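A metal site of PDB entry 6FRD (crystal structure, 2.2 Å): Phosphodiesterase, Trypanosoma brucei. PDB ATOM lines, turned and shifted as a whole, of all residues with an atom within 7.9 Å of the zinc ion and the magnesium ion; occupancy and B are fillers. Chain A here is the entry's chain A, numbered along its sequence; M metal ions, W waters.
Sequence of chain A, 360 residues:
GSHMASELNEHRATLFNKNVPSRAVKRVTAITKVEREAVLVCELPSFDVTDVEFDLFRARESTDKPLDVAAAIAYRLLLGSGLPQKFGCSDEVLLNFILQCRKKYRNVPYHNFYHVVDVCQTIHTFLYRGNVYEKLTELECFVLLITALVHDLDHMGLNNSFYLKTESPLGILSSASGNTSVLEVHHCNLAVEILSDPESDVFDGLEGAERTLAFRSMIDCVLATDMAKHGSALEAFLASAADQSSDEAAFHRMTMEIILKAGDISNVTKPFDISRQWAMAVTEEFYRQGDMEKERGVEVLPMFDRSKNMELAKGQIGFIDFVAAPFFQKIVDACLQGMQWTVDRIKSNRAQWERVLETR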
ATOM      1  N   TYR A 105       8.222  -3.084 -30.000  1.00  0.00           N
ATOM      2  CA  TYR A 105       7.252  -4.225 -29.901  1.00  0.00           C
ATOM      3  C   TYR A 105       6.273  -4.126 -31.044  1.00  0.00           C
ATOM      4  O   TYR A 105       6.002  -3.049 -31.537  1.00  0.00           O
ATOM      5  CB  TYR A 105       6.584  -4.307 -28.512  1.00  0.00           C
ATOM      6  CG  TYR A 105       7.571  -4.809 -27.489  1.00  0.00           C
ATOM      7  CD1 TYR A 105       7.865  -6.152 -27.394  1.00  0.00           C
ATOM      8  CD2 TYR A 105       8.275  -3.915 -26.684  1.00  0.00           C
ATOM      9  CE1 TYR A 105       8.824  -6.606 -26.488  1.00  0.00           C
ATOM     10  CE2 TYR A 105       9.227  -4.365 -25.783  1.00  0.00           C
ATOM     11  CZ  TYR A 105       9.507  -5.723 -25.700  1.00  0.00           C
ATOM     12  OH  TYR A 105      10.451  -6.192 -24.806  1.00  0.00           O
ATOM     13  N   TYR A 110       0.231 -11.878 -28.500  1.00  0.00           N
ATOM     14  CA  TYR A 110       0.799 -12.129 -27.159  1.00  0.00           C
ATOM     15  C   TYR A 110       2.118 -11.378 -26.837  1.00  0.00           C
ATOM     16  O   TYR A 110       2.182 -10.587 -25.895  1.00  0.00           O
ATOM     17  CB  TYR A 110       0.979 -13.638 -26.950  1.00  0.00           C
ATOM     18  CG  TYR A 110       1.511 -13.986 -25.576  1.00  0.00           C
ATOM     19  CD1 TYR A 110       0.653 -14.115 -24.502  1.00  0.00           C
ATOM     20  CD2 TYR A 110       2.852 -14.188 -25.363  1.00  0.00           C
ATOM     21  CE1 TYR A 110       1.118 -14.460 -23.254  1.00  0.00           C
ATOM     22  CE2 TYR A 110       3.334 -14.522 -24.124  1.00  0.00           C
ATOM     23  CZ  TYR A 110       2.453 -14.658 -23.046  1.00  0.00           C
ATOM     24  OH  TYR A 110       2.908 -14.957 -21.802  1.00  0.00           O
ATOM     25  N   HIS A 111       3.173 -11.672 -27.619  1.00  0.00           N
ATOM     26  CA  HIS A 111       4.538 -11.156 -27.361  1.00  0.00           C
ATOM     27  C   HIS A 111       4.670  -9.688 -27.794  1.00  0.00           C
ATOM     28  O   HIS A 111       5.507  -9.328 -28.652  1.00  0.00           O
ATOM     29  CB  HIS A 111       5.552 -12.013 -28.065  1.00  0.00           C
ATOM     30  CG  HIS A 111       5.730 -13.364 -27.464  1.00  0.00           C
ATOM     31  ND1 HIS A 111       5.172 -14.501 -27.999  1.00  0.00           N
ATOM     32  CD2 HIS A 111       6.372 -13.760 -26.332  1.00  0.00           C
ATOM     33  CE1 HIS A 111       5.492 -15.541 -27.262  1.00  0.00           C
ATOM     34  NE2 HIS A 111       6.215 -15.114 -26.236  1.00  0.00           N
ATOM     35  N   ASN A 112       3.890  -8.842 -27.121  1.00  0.00           N
ATOM     36  CA  ASN A 112       3.750  -7.441 -27.441  1.00  0.00           C
ATOM     37  C   ASN A 112       4.118  -6.634 -26.218  1.00  0.00           C
ATOM     38  O   ASN A 112       4.566  -7.183 -25.209  1.00  0.00           O
ATOM     39  CB  ASN A 112       2.293  -7.145 -27.891  1.00  0.00           C
ATOM     40  CG  ASN A 112       1.257  -7.642 -26.905  1.00  0.00           C
ATOM     41  OD1 ASN A 112       1.372  -7.407 -25.727  1.00  0.00           O
ATOM     42  ND2 ASN A 112       0.251  -8.325 -27.383  1.00  0.00           N
ATOM     43  N   HIS A 115       2.677  -7.647 -22.793  1.00  0.00           N
ATOM     44  CA  HIS A 115       3.312  -8.795 -22.167  1.00  0.00           C
ATOM     45  C   HIS A 115       4.492  -8.379 -21.316  1.00  0.00           C
ATOM     46  O   HIS A 115       4.640  -8.845 -20.199  1.00  0.00           O
ATOM     47  CB  HIS A 115       3.709  -9.835 -23.206  1.00  0.00           C
ATOM     48  CG  HIS A 115       4.718 -10.838 -22.745  1.00  0.00           C
ATOM     49  ND1 HIS A 115       4.466 -11.754 -21.754  1.00  0.00           N
ATOM     50  CD2 HIS A 115       5.953 -11.128 -23.219  1.00  0.00           C
ATOM     51  CE1 HIS A 115       5.506 -12.545 -21.615  1.00  0.00           C
ATOM     52  NE2 HIS A 115       6.424 -12.186 -22.478  1.00  0.00           N
ATOM     53  N   VAL A 116       5.320  -7.476 -21.828  1.00  0.00           N
ATOM     54  CA  VAL A 116       6.552  -7.142 -21.130  1.00  0.00           C
ATOM     55  C   VAL A 116       6.268  -6.234 -19.999  1.00  0.00           C
ATOM     56  O   VAL A 116       6.974  -6.309 -18.991  1.00  0.00           O
ATOM     57  CB  VAL A 116       7.688  -6.629 -22.047  1.00  0.00           C
ATOM     58  CG1 VAL A 116       7.991  -7.662 -23.127  1.00  0.00           C
ATOM     59  CG2 VAL A 116       7.369  -5.256 -22.660  1.00  0.00           C
ATOM     60  N   VAL A 119       5.187  -8.583 -17.400  1.00  0.00           N
ATOM     61  CA  VAL A 119       6.330  -9.290 -16.773  1.00  0.00           C
ATOM     62  C   VAL A 119       7.059  -8.384 -15.785  1.00  0.00           C
ATOM     63  O   VAL A 119       7.441  -8.820 -14.684  1.00  0.00           O
ATOM     64  CB  VAL A 119       7.290  -9.871 -17.841  1.00  0.00           C
ATOM     65  CG1 VAL A 119       8.540 -10.455 -17.186  1.00  0.00           C
ATOM     66  CG2 VAL A 119       6.585 -10.936 -18.694  1.00  0.00           C
ATOM     67  N   ALA A 148      12.970  -6.872 -17.852  1.00  0.00           N
ATOM     68  CA  ALA A 148      11.640  -7.249 -18.241  1.00  0.00           C
ATOM     69  C   ALA A 148      11.152  -6.525 -19.489  1.00  0.00           C
ATOM     70  O   ALA A 148      10.528  -7.133 -20.379  1.00  0.00           O
ATOM     71  CB  ALA A 148      10.702  -7.010 -17.079  1.00  0.00           C
ATOM     72  N   HIS A 151      12.998  -7.790 -22.827  1.00  0.00           N
ATOM     73  CA  HIS A 151      13.292  -9.219 -22.949  1.00  0.00           C
ATOM     74  C   HIS A 151      12.697  -9.897 -24.175  1.00  0.00           C
ATOM     75  O   HIS A 151      13.113 -11.032 -24.488  1.00  0.00           O
ATOM     76  CB  HIS A 151      12.914 -10.005 -21.669  1.00  0.00           C
ATOM     77  CG  HIS A 151      11.494 -10.498 -21.630  1.00  0.00           C
ATOM     78  ND1 HIS A 151      10.449  -9.708 -21.195  1.00  0.00           N
ATOM     79  CD2 HIS A 151      10.958 -11.685 -21.977  1.00  0.00           C
ATOM     80  CE1 HIS A 151       9.322 -10.398 -21.296  1.00  0.00           C
ATOM     81  NE2 HIS A 151       9.599 -11.595 -21.789  1.00  0.00           N
ATOM     82  N   ASP A 152      11.745  -9.271 -24.856  1.00  0.00           N
ATOM     83  CA  ASP A 152      11.146  -9.805 -26.084  1.00  0.00           C
ATOM     84  C   ASP A 152      11.149  -8.784 -27.240  1.00  0.00           C
ATOM     85  O   ASP A 152      10.285  -8.855 -28.155  1.00  0.00           O
ATOM     86  CB  ASP A 152       9.686 -10.273 -25.867  1.00  0.00           C
ATOM     87  CG  ASP A 152       9.568 -11.646 -25.276  1.00  0.00           C
ATOM     88  OD1 ASP A 152      10.342 -12.571 -25.634  1.00  0.00           O
ATOM     89  OD2 ASP A 152       8.609 -11.813 -24.486  1.00  0.00           O
ATOM     90  N   LEU A 153      12.101  -7.836 -27.233  1.00  0.00           N
ATOM     91  CA  LEU A 153      12.081  -6.751 -28.196  1.00  0.00           C
ATOM     92  C   LEU A 153      11.956  -7.296 -29.603  1.00  0.00           C
ATOM     93  O   LEU A 153      12.688  -8.251 -29.955  1.00  0.00           O
ATOM     94  CB  LEU A 153      13.328  -5.901 -28.104  1.00  0.00           C
ATOM     95  CG  LEU A 153      13.342  -4.910 -26.969  1.00  0.00           C
ATOM     96  CD1 LEU A 153      14.784  -4.514 -26.655  1.00  0.00           C
ATOM     97  CD2 LEU A 153      12.536  -3.669 -27.284  1.00  0.00           C
ATOM     98  N   HIS A 155       9.753  -9.166 -31.058  1.00  0.00           N
ATOM     99  CA  HIS A 155       9.177 -10.496 -31.237  1.00  0.00           C
ATOM    100  C   HIS A 155       8.122 -10.396 -32.345  1.00  0.00           C
ATOM    101  O   HIS A 155       7.350  -9.425 -32.387  1.00  0.00           O
ATOM    102  CB  HIS A 155       8.502 -10.993 -29.943  1.00  0.00           C
ATOM    103  CG  HIS A 155       8.453 -12.468 -29.825  1.00  0.00           C
ATOM    104  ND1 HIS A 155       7.680 -13.272 -30.652  1.00  0.00           N
ATOM    105  CD2 HIS A 155       9.081 -13.330 -28.954  1.00  0.00           C
ATOM    106  CE1 HIS A 155       7.832 -14.539 -30.310  1.00  0.00           C
ATOM    107  NE2 HIS A 155       8.703 -14.617 -29.300  1.00  0.00           N
ATOM    108  N   ASN A 160      11.614 -19.972 -31.796  1.00  0.00           N
ATOM    109  CA  ASN A 160      12.910 -20.327 -32.303  1.00  0.00           C
ATOM    110  C   ASN A 160      12.842 -21.455 -33.318  1.00  0.00           C
ATOM    111  O   ASN A 160      13.544 -21.415 -34.341  1.00  0.00           O
ATOM    112  CB  ASN A 160      13.884 -20.691 -31.159  1.00  0.00           C
ATOM    113  CG  ASN A 160      14.347 -19.491 -30.371  1.00  0.00           C
ATOM    114  OD1 ASN A 160      14.319 -18.351 -30.866  1.00  0.00           O
ATOM    115  ND2 ASN A 160      14.784 -19.736 -29.116  1.00  0.00           N
ATOM    116  N   LEU A 183      15.887 -15.933 -31.134  1.00  0.00           N
ATOM    117  CA  LEU A 183      15.184 -14.724 -30.701  1.00  0.00           C
ATOM    118  C   LEU A 183      15.827 -14.000 -29.525  1.00  0.00           C
ATOM    119  O   LEU A 183      15.917 -12.750 -29.527  1.00  0.00           O
ATOM    120  CB  LEU A 183      13.781 -15.055 -30.338  1.00  0.00           C
ATOM    121  CG  LEU A 183      12.926 -15.208 -31.594  1.00  0.00           C
ATOM    122  CD1 LEU A 183      11.619 -15.829 -31.176  1.00  0.00           C
ATOM    123  CD2 LEU A 183      12.677 -13.863 -32.305  1.00  0.00           C
ATOM    124  N   GLU A 184      16.303 -14.767 -28.548  1.00  0.00           N
ATOM    125  CA  GLU A 184      16.830 -14.175 -27.313  1.00  0.00           C
ATOM    126  C   GLU A 184      18.065 -13.334 -27.649  1.00  0.00           C
ATOM    127  O   GLU A 184      18.207 -12.202 -27.147  1.00  0.00           O
ATOM    128  CB  GLU A 184      17.099 -15.270 -26.261  1.00  0.00           C
ATOM    129  CG  GLU A 184      15.834 -15.924 -25.715  1.00  0.00           C
ATOM    130  CD  GLU A 184      15.100 -16.875 -26.682  1.00  0.00           C
ATOM    131  OE1 GLU A 184      15.711 -17.436 -27.635  1.00  0.00           O
ATOM    132  OE2 GLU A 184      13.871 -17.080 -26.480  1.00  0.00           O
ATOM    133  N   HIS A 187      16.800 -10.186 -29.200  1.00  0.00           N
ATOM    134  CA  HIS A 187      16.309  -9.229 -28.205  1.00  0.00           C
ATOM    135  C   HIS A 187      17.468  -8.490 -27.500  1.00  0.00           C
ATOM    136  O   HIS A 187      17.404  -7.262 -27.284  1.00  0.00           O
ATOM    137  CB  HIS A 187      15.416  -9.880 -27.110  1.00  0.00           C
ATOM    138  CG  HIS A 187      14.319 -10.753 -27.636  1.00  0.00           C
ATOM    139  ND1 HIS A 187      13.480 -10.341 -28.657  1.00  0.00           N
ATOM    140  CD2 HIS A 187      13.942 -12.010 -27.308  1.00  0.00           C
ATOM    141  CE1 HIS A 187      12.624 -11.316 -28.924  1.00  0.00           C
ATOM    142  NE2 HIS A 187      12.891 -12.345 -28.121  1.00  0.00           N
ATOM    143  N   VAL A 222      18.036 -12.496 -20.226  1.00  0.00           N
ATOM    144  CA  VAL A 222      17.281 -12.611 -21.460  1.00  0.00           C
ATOM    145  C   VAL A 222      17.616 -13.914 -22.166  1.00  0.00           C
ATOM    146  O   VAL A 222      16.736 -14.609 -22.658  1.00  0.00           O
ATOM    147  CB  VAL A 222      17.565 -11.456 -22.386  1.00  0.00           C
ATOM    148  CG1 VAL A 222      16.894 -11.676 -23.744  1.00  0.00           C
ATOM    149  CG2 VAL A 222      17.001 -10.210 -21.759  1.00  0.00           C
ATOM    150  N   THR A 225      15.686 -16.890 -20.894  1.00  0.00           N
ATOM    151  CA  THR A 225      14.276 -17.091 -21.193  1.00  0.00           C
ATOM    152  C   THR A 225      13.949 -18.111 -22.293  1.00  0.00           C
ATOM    153  O   THR A 225      12.773 -18.436 -22.476  1.00  0.00           O
ATOM    154  CB  THR A 225      13.585 -15.764 -21.518  1.00  0.00           C
ATOM    155  OG1 THR A 225      14.133 -15.192 -22.681  1.00  0.00           O
ATOM    156  CG2 THR A 225      13.731 -14.823 -20.348  1.00  0.00           C
ATOM    157  N   ASP A 226      14.957 -18.628 -22.994  1.00  0.00           N
ATOM    158  CA  ASP A 226      14.754 -19.641 -24.056  1.00  0.00           C
ATOM    159  C   ASP A 226      14.319 -20.945 -23.382  1.00  0.00           C
ATOM    160  O   ASP A 226      15.080 -21.561 -22.584  1.00  0.00           O
ATOM    161  CB  ASP A 226      16.067 -19.858 -24.827  1.00  0.00           C
ATOM    162  CG  ASP A 226      15.961 -20.925 -25.921  1.00  0.00           C
ATOM    163  OD1 ASP A 226      14.982 -21.654 -25.996  1.00  0.00           O
ATOM    164  OD2 ASP A 226      16.903 -21.040 -26.708  1.00  0.00           O
ATOM    165  N   MET A 227      13.115 -21.389 -23.693  1.00  0.00           N
ATOM    166  CA  MET A 227      12.560 -22.562 -23.054  1.00  0.00           C
ATOM    167  C   MET A 227      13.298 -23.871 -23.303  1.00  0.00           C
ATOM    168  O   MET A 227      13.172 -24.792 -22.504  1.00  0.00           O
ATOM    169  CB  MET A 227      11.061 -22.717 -23.338  1.00  0.00           C
ATOM    170  CG  MET A 227      10.196 -21.712 -22.532  1.00  0.00           C
ATOM    171  SD  MET A 227      10.384 -21.750 -20.693  1.00  0.00           S
ATOM    172  CE  MET A 227       9.570 -23.298 -20.345  1.00  0.00           C
ATOM    173  N   LEU A 260      13.298 -13.739 -13.799  1.00  0.00           N
ATOM    174  CA  LEU A 260      12.808 -13.342 -15.113  1.00  0.00           C
ATOM    175  C   LEU A 260      12.069 -14.499 -15.748  1.00  0.00           C
ATOM    176  O   LEU A 260      11.000 -14.330 -16.286  1.00  0.00           O
ATOM    177  CB  LEU A 260      13.932 -12.844 -16.027  1.00  0.00           C
ATOM    178  CG  LEU A 260      13.430 -12.433 -17.418  1.00  0.00           C
ATOM    179  CD1 LEU A 260      12.534 -11.209 -17.347  1.00  0.00           C
ATOM    180  CD2 LEU A 260      14.574 -12.141 -18.313  1.00  0.00           C
ATOM    181  N   LYS A 261      12.618 -15.698 -15.654  1.00  0.00           N
ATOM    182  CA  LYS A 261      11.907 -16.896 -16.101  1.00  0.00           C
ATOM    183  C   LYS A 261      10.527 -17.025 -15.458  1.00  0.00           C
ATOM    184  O   LYS A 261       9.559 -17.224 -16.173  1.00  0.00           O
ATOM    185  CB  LYS A 261      12.688 -18.175 -15.854  1.00  0.00           C
ATOM    186  CG  LYS A 261      13.814 -18.417 -16.825  1.00  0.00           C
ATOM    187  CD  LYS A 261      14.516 -19.760 -16.574  1.00  0.00           C
ATOM    188  CE  LYS A 261      13.582 -20.987 -16.649  1.00  0.00           C
ATOM    189  NZ  LYS A 261      12.719 -21.069 -17.908  1.00  0.00           N
ATOM    190  N   GLY A 263       8.584 -14.665 -14.096  1.00  0.00           N
ATOM    191  CA  GLY A 263       7.727 -13.639 -14.638  1.00  0.00           C
ATOM    192  C   GLY A 263       7.203 -13.979 -16.017  1.00  0.00           C
ATOM    193  O   GLY A 263       6.064 -13.731 -16.334  1.00  0.00           O
ATOM    194  N   ASP A 264       8.053 -14.561 -16.830  1.00  0.00           N
ATOM    195  CA  ASP A 264       7.764 -14.909 -18.205  1.00  0.00           C
ATOM    196  C   ASP A 264       6.689 -16.015 -18.332  1.00  0.00           C
ATOM    197  O   ASP A 264       5.906 -15.985 -19.257  1.00  0.00           O
ATOM    198  CB  ASP A 264       9.051 -15.329 -18.920  1.00  0.00           C
ATOM    199  CG  ASP A 264       9.012 -14.991 -20.424  1.00  0.00           C
ATOM    200  OD1 ASP A 264       8.245 -14.099 -20.834  1.00  0.00           O
ATOM    201  OD2 ASP A 264       9.725 -15.614 -21.201  1.00  0.00           O
ATOM    202  N   ILE A 265       6.650 -16.952 -17.391  1.00  0.00           N
ATOM    203  CA  ILE A 265       5.622 -17.990 -17.366  1.00  0.00           C
ATOM    204  C   ILE A 265       4.632 -17.801 -16.218  1.00  0.00           C
ATOM    205  O   ILE A 265       4.054 -18.753 -15.734  1.00  0.00           O
ATOM    206  CB  ILE A 265       6.239 -19.402 -17.311  1.00  0.00           C
ATOM    207  CG1 ILE A 265       7.024 -19.639 -16.012  1.00  0.00           C
ATOM    208  CG2 ILE A 265       7.169 -19.612 -18.493  1.00  0.00           C
ATOM    209  CD1 ILE A 265       7.507 -21.044 -15.820  1.00  0.00           C
HETATM  210 ZN    ZN M   1       8.400 -13.153 -22.783  1.00  0.00          ZN
HETATM  211 MG    MG M   2      11.038 -14.656 -25.280  1.00  0.00          MG
HETATM  212  O   HOH W   1      12.109 -16.417 -24.470  1.00  0.00           O
HETATM  213  O   HOH W   2      11.801 -14.592 -27.223  1.00  0.00           O
HETATM  214  O   HOH W   3       9.160 -15.644 -25.876  1.00  0.00           O
HETATM  215  O   HOH W   4       7.053 -15.167 -23.614  1.00  0.00           O
HETATM  216  O   HOH W   5      12.737 -13.823 -24.459  1.00  0.00           O
HETATM  217  O   HOH W   6       9.899 -14.366 -23.439  1.00  0.00           O
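Water W6 binds the zinc ion (2.0 Å).
The zinc ion is bound by OD1 of Asp 264 (2.2 Å).
The zinc ion is bound by the side-chain carboxylate (OD2) of Asp 152.
The zinc ion is bound by NE2 of His 151 (2.2 Å).
The zinc ion is bound by NE2 of His 115.
Water W4 binds the zinc ion.
The zinc ion has six donor atoms within binding distance.
Within 4 Å of the zinc ion: His 115, His 151, Asp 152 and Asp 264.
OE1 of Glu 184 is in hydrogen-bond range of ND2 of Asn 160 (2.9 Å).
The side-chain hydroxyl of Tyr 105 sits at hydrogen-bond distance from the backbone NH of Asp 152 (3.3 Å).
The backbone NH of His 115 sits at hydrogen-bond distance from the side-chain amide oxygen of Asn 112 (3.2 Å).
ND1 of His 151 sits at hydrogen-bond distance from O of Ala 148, 2.7 Å away.
The magnesium ion is bound by water W5, water W2, water W6, water W3, water W1 and OD1 of Asp 152.
The magnesium ion has six donor atoms within binding distance.
Water W2 lies within hydrogen-bond range of a ring nitrogen (NE2) of His 187 and the side-chain carboxylate (OE2) of Glu 184.
Water W5 lies within hydrogen-bond range of the side-chain hydroxyl of Thr 225 (2.6 Å) and the backbone carbonyl oxygen of His 151 (2.8 Å).
Water W1 bridges OE2 of Glu 184 and O of Thr 225.
OE2 of Glu 184 touches the magnesium ion (3.9 Å).
Two residues have an atom within 4 Å of the magnesium ion: Asp 152 and Glu 184.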
